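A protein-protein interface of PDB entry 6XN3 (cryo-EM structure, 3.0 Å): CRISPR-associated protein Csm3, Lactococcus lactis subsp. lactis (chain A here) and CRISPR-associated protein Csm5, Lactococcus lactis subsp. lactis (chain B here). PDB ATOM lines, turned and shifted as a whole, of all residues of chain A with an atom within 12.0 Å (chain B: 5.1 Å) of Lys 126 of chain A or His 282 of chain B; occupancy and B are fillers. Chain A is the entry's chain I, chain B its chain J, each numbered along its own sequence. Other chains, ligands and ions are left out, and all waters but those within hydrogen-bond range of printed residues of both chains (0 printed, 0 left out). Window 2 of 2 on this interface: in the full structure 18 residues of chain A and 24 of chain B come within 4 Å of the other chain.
Among the printed residues, merely in contact across the chains: Lys 126 of chain A with His 282 of chain B (3.1 Å), Thr 127 of chain A with Asp 297 of chain B (3.3 Å), Arg 125 of chain A with Thr 280 of chain B (3.4 Å), Arg 125 of chain A with Leu 281 of chain B (3.6 Å), Ala 128 of chain A with Phe 276 of chain B (3.6 Å), Arg 125 of chain A with His 282 of chain B (3.6 Å), Lys 126 of chain A with Asp 297 of chain B (3.8 Å) and Ala 128 of chain A with Thr 280 of chain B (3.9 Å).
Hydrophobic or aromatic side chains of chain B that line the printed part of chain A: Phe 276, Leu 281 and His 282. Of the 10 printed residues of chain A, 4 touch a printed residue of chain B. Hydrophobic or aromatic side chains of chain A that line the printed part of chain B: Ala 128. Among the printed residues, 8 pairs touch across the chains. Among the printed residues, no Asp or Glu carboxylate lies within 4 Å of a Lys or Arg side-chain nitrogen of the other chain.
Ile 123 of chain A touches none of the printed residues of chain B. Asn 124 of chain A touches none of the printed residues of chain B. Of the printed residues of chain B, Arg 125 of chain A touches Thr 280 (3.4 Å), Leu 281 (3.6 Å) and His 282 (3.6 Å). Of chain B, only His 282 (3.1 Å) and Asp 297 (3.8 Å) come within 4 Å of Lys 126 of chain A. Printed residues of chain B within 4 Å of Thr 127 of chain A: Asp 297. Of the printed residues of chain B, Ala 128 of chain A touches Phe 276 (3.6 Å) and Thr 280 (3.9 Å). Printed residues of chain A within 4 Å of Phe 276 of chain B: Ala 128 (3.6 Å). Of the printed residues of chain A, Thr 280 of chain B touches Arg 125 and Ala 128. Leu 281 of chain B touches just one residue of chain A: Arg 125. Tyr 283 of chain B touches none of the printed residues of chain A. No residue of chain A comes within 4 Å of Asp 294 of chain B. Asp 297 of chain B touches just these residues of chain A: Lys 126 (3.8 Å) and Thr 127 (3.3 Å).
OD1 of Asn 124 of chain A sits at hydrogen-bond distance from N of Lys 126 of chain A. The backbone carbonyl oxygen of Phe 276 of chain B sits at hydrogen-bond distance from the side-chain hydroxyl of Thr 280 of chain B, 3.0 Å away. The backbone carbonyl oxygen of His 282 of chain B sits close to the side-chain amide oxygen of Gln 290 of chain B.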
ATOM      1  N   THR A 122      33.783 -14.279   1.935  1.00  0.00           N
ATOM      2  CA  THR A 122      32.455 -13.739   2.158  1.00  0.00           C
ATOM      3  C   THR A 122      32.487 -12.256   1.852  1.00  0.00           C
ATOM      4  O   THR A 122      33.260 -11.515   2.461  1.00  0.00           O
ATOM      5  CB  THR A 122      31.994 -13.961   3.592  1.00  0.00           C
ATOM      6  OG1 THR A 122      32.155 -15.341   3.932  1.00  0.00           O
ATOM      7  CG2 THR A 122      30.541 -13.572   3.741  1.00  0.00           C
ATOM      8  N   ILE A 123      31.651 -11.825   0.920  1.00  0.00           N
ATOM      9  CA  ILE A 123      31.527 -10.419   0.576  1.00  0.00           C
ATOM     10  C   ILE A 123      30.431  -9.825   1.437  1.00  0.00           C
ATOM     11  O   ILE A 123      29.263 -10.211   1.318  1.00  0.00           O
ATOM     12  CB  ILE A 123      31.227 -10.217  -0.912  1.00  0.00           C
ATOM     13  CG1 ILE A 123      32.389 -10.735  -1.751  1.00  0.00           C
ATOM     14  CG2 ILE A 123      30.937  -8.763  -1.201  1.00  0.00           C
ATOM     15  CD1 ILE A 123      32.083 -10.811  -3.210  1.00  0.00           C
ATOM     16  N   ASN A 124      30.811  -8.902   2.314  1.00  0.00           N
ATOM     17  CA  ASN A 124      29.838  -8.135   3.074  1.00  0.00           C
ATOM     18  C   ASN A 124      29.210  -7.211   2.046  1.00  0.00           C
ATOM     19  O   ASN A 124      29.905  -6.397   1.439  1.00  0.00           O
ATOM     20  CB  ASN A 124      30.549  -7.391   4.216  1.00  0.00           C
ATOM     21  CG  ASN A 124      29.698  -6.306   4.949  1.00  0.00           C
ATOM     22  OD1 ASN A 124      28.623  -5.866   4.539  1.00  0.00           O
ATOM     23  ND2 ASN A 124      30.240  -5.868   6.076  1.00  0.00           N
ATOM     24  N   ARG A 125      27.899  -7.318   1.868  1.00  0.00           N
ATOM     25  CA  ARG A 125      27.264  -6.643   0.748  1.00  0.00           C
ATOM     26  C   ARG A 125      27.106  -5.144   0.955  1.00  0.00           C
ATOM     27  O   ARG A 125      26.679  -4.451   0.027  1.00  0.00           O
ATOM     28  CB  ARG A 125      25.905  -7.273   0.470  1.00  0.00           C
ATOM     29  CG  ARG A 125      25.927  -8.435  -0.488  1.00  0.00           C
ATOM     30  CD  ARG A 125      26.155  -9.747   0.223  1.00  0.00           C
ATOM     31  NE  ARG A 125      26.261 -10.845  -0.728  1.00  0.00           N
ATOM     32  CZ  ARG A 125      25.220 -11.497  -1.230  1.00  0.00           C
ATOM     33  NH1 ARG A 125      23.989 -11.162  -0.870  1.00  0.00           N
ATOM     34  NH2 ARG A 125      25.409 -12.478  -2.098  1.00  0.00           N
ATOM     35  N   LYS A 126      27.432  -4.628   2.137  1.00  0.00           N
ATOM     36  CA  LYS A 126      27.341  -3.194   2.366  1.00  0.00           C
ATOM     37  C   LYS A 126      28.506  -2.463   1.719  1.00  0.00           C
ATOM     38  O   LYS A 126      28.306  -1.565   0.898  1.00  0.00           O
ATOM     39  CB  LYS A 126      27.295  -2.913   3.869  1.00  0.00           C
ATOM     40  CG  LYS A 126      26.522  -1.668   4.270  1.00  0.00           C
ATOM     41  CD  LYS A 126      26.715  -1.376   5.751  1.00  0.00           C
ATOM     42  CE  LYS A 126      26.120  -0.039   6.147  1.00  0.00           C
ATOM     43  NZ  LYS A 126      27.103   1.073   6.029  1.00  0.00           N
ATOM     44  N   THR A 127      29.731  -2.836   2.070  1.00  0.00           N
ATOM     45  CA  THR A 127      30.909  -2.125   1.608  1.00  0.00           C
ATOM     46  C   THR A 127      31.775  -2.936   0.660  1.00  0.00           C
ATOM     47  O   THR A 127      32.843  -2.451   0.270  1.00  0.00           O
ATOM     48  CB  THR A 127      31.757  -1.686   2.807  1.00  0.00           C
ATOM     49  OG1 THR A 127      32.189  -2.845   3.523  1.00  0.00           O
ATOM     50  CG2 THR A 127      30.936  -0.824   3.747  1.00  0.00           C
ATOM     51  N   ALA A 128      31.350  -4.154   0.308  1.00  0.00           N
ATOM     52  CA  ALA A 128      32.013  -5.047  -0.649  1.00  0.00           C
ATOM     53  C   ALA A 128      33.442  -5.394  -0.246  1.00  0.00           C
ATOM     54  O   ALA A 128      34.290  -5.650  -1.101  1.00  0.00           O
ATOM     55  CB  ALA A 128      31.981  -4.480  -2.070  1.00  0.00           C
ATOM     56  N   VAL A 129      33.725  -5.424   1.051  1.00  0.00           N
ATOM     57  CA  VAL A 129      35.014  -5.884   1.545  1.00  0.00           C
ATOM     58  C   VAL A 129      34.880  -7.365   1.869  1.00  0.00           C
ATOM     59  O   VAL A 129      33.856  -7.814   2.399  1.00  0.00           O
ATOM     60  CB  VAL A 129      35.500  -5.049   2.753  1.00  0.00           C
ATOM     61  CG1 VAL A 129      34.530  -5.090   3.920  1.00  0.00           C
ATOM     62  CG2 VAL A 129      36.898  -5.461   3.186  1.00  0.00           C
ATOM     63  N   ALA A 130      35.875  -8.144   1.472  1.00  0.00           N
ATOM     64  CA  ALA A 130      35.772  -9.586   1.565  1.00  0.00           C
ATOM     65  C   ALA A 130      36.230 -10.074   2.935  1.00  0.00           C
ATOM     66  O   ALA A 130      36.596  -9.296   3.816  1.00  0.00           O
ATOM     67  CB  ALA A 130      36.570 -10.246   0.448  1.00  0.00           C
ATOM     68  N   ASN A 131      36.203 -11.387   3.108  1.00  0.00           N
ATOM     69  CA  ASN A 131      36.516 -12.058   4.361  1.00  0.00           C
ATOM     70  C   ASN A 131      36.908 -13.492   4.040  1.00  0.00           C
ATOM     71  O   ASN A 131      36.051 -14.380   4.039  1.00  0.00           O
ATOM     72  CB  ASN A 131      35.314 -11.998   5.299  1.00  0.00           C
ATOM     73  CG  ASN A 131      35.570 -12.668   6.622  1.00  0.00           C
ATOM     74  OD1 ASN A 131      34.819 -13.548   7.034  1.00  0.00           O
ATOM     75  ND2 ASN A 131      36.633 -12.259   7.301  1.00  0.00           N
ATOM     76  N   LYS B 144      18.372  -4.940   2.687  1.00  0.00           N
ATOM     77  CA  LYS B 144      19.564  -5.602   3.213  1.00  0.00           C
ATOM     78  C   LYS B 144      19.370  -5.810   4.712  1.00  0.00           C
ATOM     79  O   LYS B 144      19.882  -5.075   5.559  1.00  0.00           O
ATOM     80  CB  LYS B 144      20.813  -4.785   2.919  1.00  0.00           C
ATOM     81  CG  LYS B 144      22.105  -5.507   3.249  1.00  0.00           C
ATOM     82  CD  LYS B 144      23.238  -4.532   3.466  1.00  0.00           C
ATOM     83  CE  LYS B 144      23.245  -4.021   4.885  1.00  0.00           C
ATOM     84  NZ  LYS B 144      23.673  -5.077   5.839  1.00  0.00           N
ATOM     85  N   PHE B 276      31.649  -3.246  -8.523  1.00  0.00           N
ATOM     86  CA  PHE B 276      31.163  -3.029  -7.166  1.00  0.00           C
ATOM     87  C   PHE B 276      29.654  -3.195  -7.088  1.00  0.00           C
ATOM     88  O   PHE B 276      29.138  -3.841  -6.171  1.00  0.00           O
ATOM     89  CB  PHE B 276      31.587  -1.635  -6.698  1.00  0.00           C
ATOM     90  CG  PHE B 276      30.917  -1.180  -5.441  1.00  0.00           C
ATOM     91  CD1 PHE B 276      31.356  -1.635  -4.215  1.00  0.00           C
ATOM     92  CD2 PHE B 276      29.854  -0.294  -5.481  1.00  0.00           C
ATOM     93  CE1 PHE B 276      30.745  -1.230  -3.058  1.00  0.00           C
ATOM     94  CE2 PHE B 276      29.242   0.109  -4.327  1.00  0.00           C
ATOM     95  CZ  PHE B 276      29.689  -0.354  -3.113  1.00  0.00           C
ATOM     96  N   THR B 280      27.399  -5.876  -4.705  1.00  0.00           N
ATOM     97  CA  THR B 280      26.525  -5.362  -3.671  1.00  0.00           C
ATOM     98  C   THR B 280      25.071  -5.567  -4.064  1.00  0.00           C
ATOM     99  O   THR B 280      24.745  -6.238  -5.045  1.00  0.00           O
ATOM    100  CB  THR B 280      26.807  -3.889  -3.423  1.00  0.00           C
ATOM    101  OG1 THR B 280      26.656  -3.167  -4.648  1.00  0.00           O
ATOM    102  CG2 THR B 280      28.210  -3.726  -2.927  1.00  0.00           C
ATOM    103  N   LEU B 281      24.178  -4.968  -3.292  1.00  0.00           N
ATOM    104  CA  LEU B 281      22.754  -5.082  -3.557  1.00  0.00           C
ATOM    105  C   LEU B 281      22.095  -3.720  -3.503  1.00  0.00           C
ATOM    106  O   LEU B 281      20.958  -3.574  -3.964  1.00  0.00           O
ATOM    107  CB  LEU B 281      22.054  -5.992  -2.543  1.00  0.00           C
ATOM    108  CG  LEU B 281      21.823  -5.444  -1.125  1.00  0.00           C
ATOM    109  CD1 LEU B 281      20.823  -6.311  -0.407  1.00  0.00           C
ATOM    110  CD2 LEU B 281      23.031  -5.227  -0.260  1.00  0.00           C
ATOM    111  N   HIS B 282      22.771  -2.719  -2.954  1.00  0.00           N
ATOM    112  CA  HIS B 282      22.089  -1.485  -2.588  1.00  0.00           C
ATOM    113  C   HIS B 282      22.058  -0.474  -3.727  1.00  0.00           C
ATOM    114  O   HIS B 282      22.472   0.671  -3.612  1.00  0.00           O
ATOM    115  CB  HIS B 282      22.690  -0.912  -1.305  1.00  0.00           C
ATOM    116  CG  HIS B 282      24.133  -0.533  -1.398  1.00  0.00           C
ATOM    117  ND1 HIS B 282      25.150  -1.457  -1.309  1.00  0.00           N
ATOM    118  CD2 HIS B 282      24.732   0.675  -1.504  1.00  0.00           C
ATOM    119  CE1 HIS B 282      26.312  -0.838  -1.396  1.00  0.00           C
ATOM    120  NE2 HIS B 282      26.086   0.456  -1.508  1.00  0.00           N
ATOM    121  N   TYR B 283      21.534  -0.932  -4.861  1.00  0.00           N
ATOM    122  CA  TYR B 283      20.695  -0.112  -5.719  1.00  0.00           C
ATOM    123  C   TYR B 283      19.223  -0.438  -5.519  1.00  0.00           C
ATOM    124  O   TYR B 283      18.465  -0.529  -6.489  1.00  0.00           O
ATOM    125  CB  TYR B 283      21.099  -0.209  -7.189  1.00  0.00           C
ATOM    126  CG  TYR B 283      22.350   0.579  -7.503  1.00  0.00           C
ATOM    127  CD1 TYR B 283      22.841   1.515  -6.605  1.00  0.00           C
ATOM    128  CD2 TYR B 283      22.991   0.450  -8.718  1.00  0.00           C
ATOM    129  CE1 TYR B 283      23.961   2.259  -6.881  1.00  0.00           C
ATOM    130  CE2 TYR B 283      24.116   1.197  -9.006  1.00  0.00           C
ATOM    131  CZ  TYR B 283      24.594   2.098  -8.083  1.00  0.00           C
ATOM    132  OH  TYR B 283      25.711   2.844  -8.359  1.00  0.00           O
ATOM    133  N   LYS B 284      18.830  -0.654  -4.266  1.00  0.00           N
ATOM    134  CA  LYS B 284      17.445  -0.610  -3.826  1.00  0.00           C
ATOM    135  C   LYS B 284      17.291   0.631  -2.949  1.00  0.00           C
ATOM    136  O   LYS B 284      18.045   0.792  -1.984  1.00  0.00           O
ATOM    137  CB  LYS B 284      17.098  -1.861  -3.021  1.00  0.00           C
ATOM    138  CG  LYS B 284      17.239  -3.227  -3.709  1.00  0.00           C
ATOM    139  CD  LYS B 284      16.227  -3.563  -4.794  1.00  0.00           C
ATOM    140  CE  LYS B 284      16.679  -3.237  -6.201  1.00  0.00           C
ATOM    141  NZ  LYS B 284      15.658  -3.714  -7.156  1.00  0.00           N
ATOM    142  N   GLN B 290      21.103   6.038  -3.336  1.00  0.00           N
ATOM    143  CA  GLN B 290      22.012   4.905  -3.274  1.00  0.00           C
ATOM    144  C   GLN B 290      23.333   5.214  -3.973  1.00  0.00           C
ATOM    145  O   GLN B 290      24.398   4.777  -3.516  1.00  0.00           O
ATOM    146  CB  GLN B 290      21.338   3.677  -3.875  1.00  0.00           C
ATOM    147  CG  GLN B 290      20.084   3.249  -3.117  1.00  0.00           C
ATOM    148  CD  GLN B 290      20.366   2.808  -1.687  1.00  0.00           C
ATOM    149  OE1 GLN B 290      21.375   2.169  -1.400  1.00  0.00           O
ATOM    150  NE2 GLN B 290      19.453   3.137  -0.785  1.00  0.00           N
ATOM    151  N   ASP B 294      26.792   5.004  -1.831  1.00  0.00           N
ATOM    152  CA  ASP B 294      27.989   4.208  -2.057  1.00  0.00           C
ATOM    153  C   ASP B 294      29.124   5.047  -2.627  1.00  0.00           C
ATOM    154  O   ASP B 294      30.286   4.662  -2.478  1.00  0.00           O
ATOM    155  CB  ASP B 294      27.698   2.967  -2.908  1.00  0.00           C
ATOM    156  CG  ASP B 294      27.209   3.265  -4.306  1.00  0.00           C
ATOM    157  OD1 ASP B 294      27.027   4.422  -4.681  1.00  0.00           O
ATOM    158  OD2 ASP B 294      27.005   2.294  -5.062  1.00  0.00           O
ATOM    159  N   ASP B 297      30.650   6.030   0.448  1.00  0.00           N
ATOM    160  CA  ASP B 297      31.054   4.840   1.188  1.00  0.00           C
ATOM    161  C   ASP B 297      32.344   4.232   0.655  1.00  0.00           C
ATOM    162  O   ASP B 297      33.189   3.784   1.434  1.00  0.00           O
ATOM    163  CB  ASP B 297      29.929   3.811   1.151  1.00  0.00           C
ATOM    164  CG  ASP B 297      30.356   2.476   1.691  1.00  0.00           C
ATOM    165  OD1 ASP B 297      30.562   2.378   2.916  1.00  0.00           O
ATOM    166  OD2 ASP B 297      30.500   1.531   0.892  1.00  0.00           O
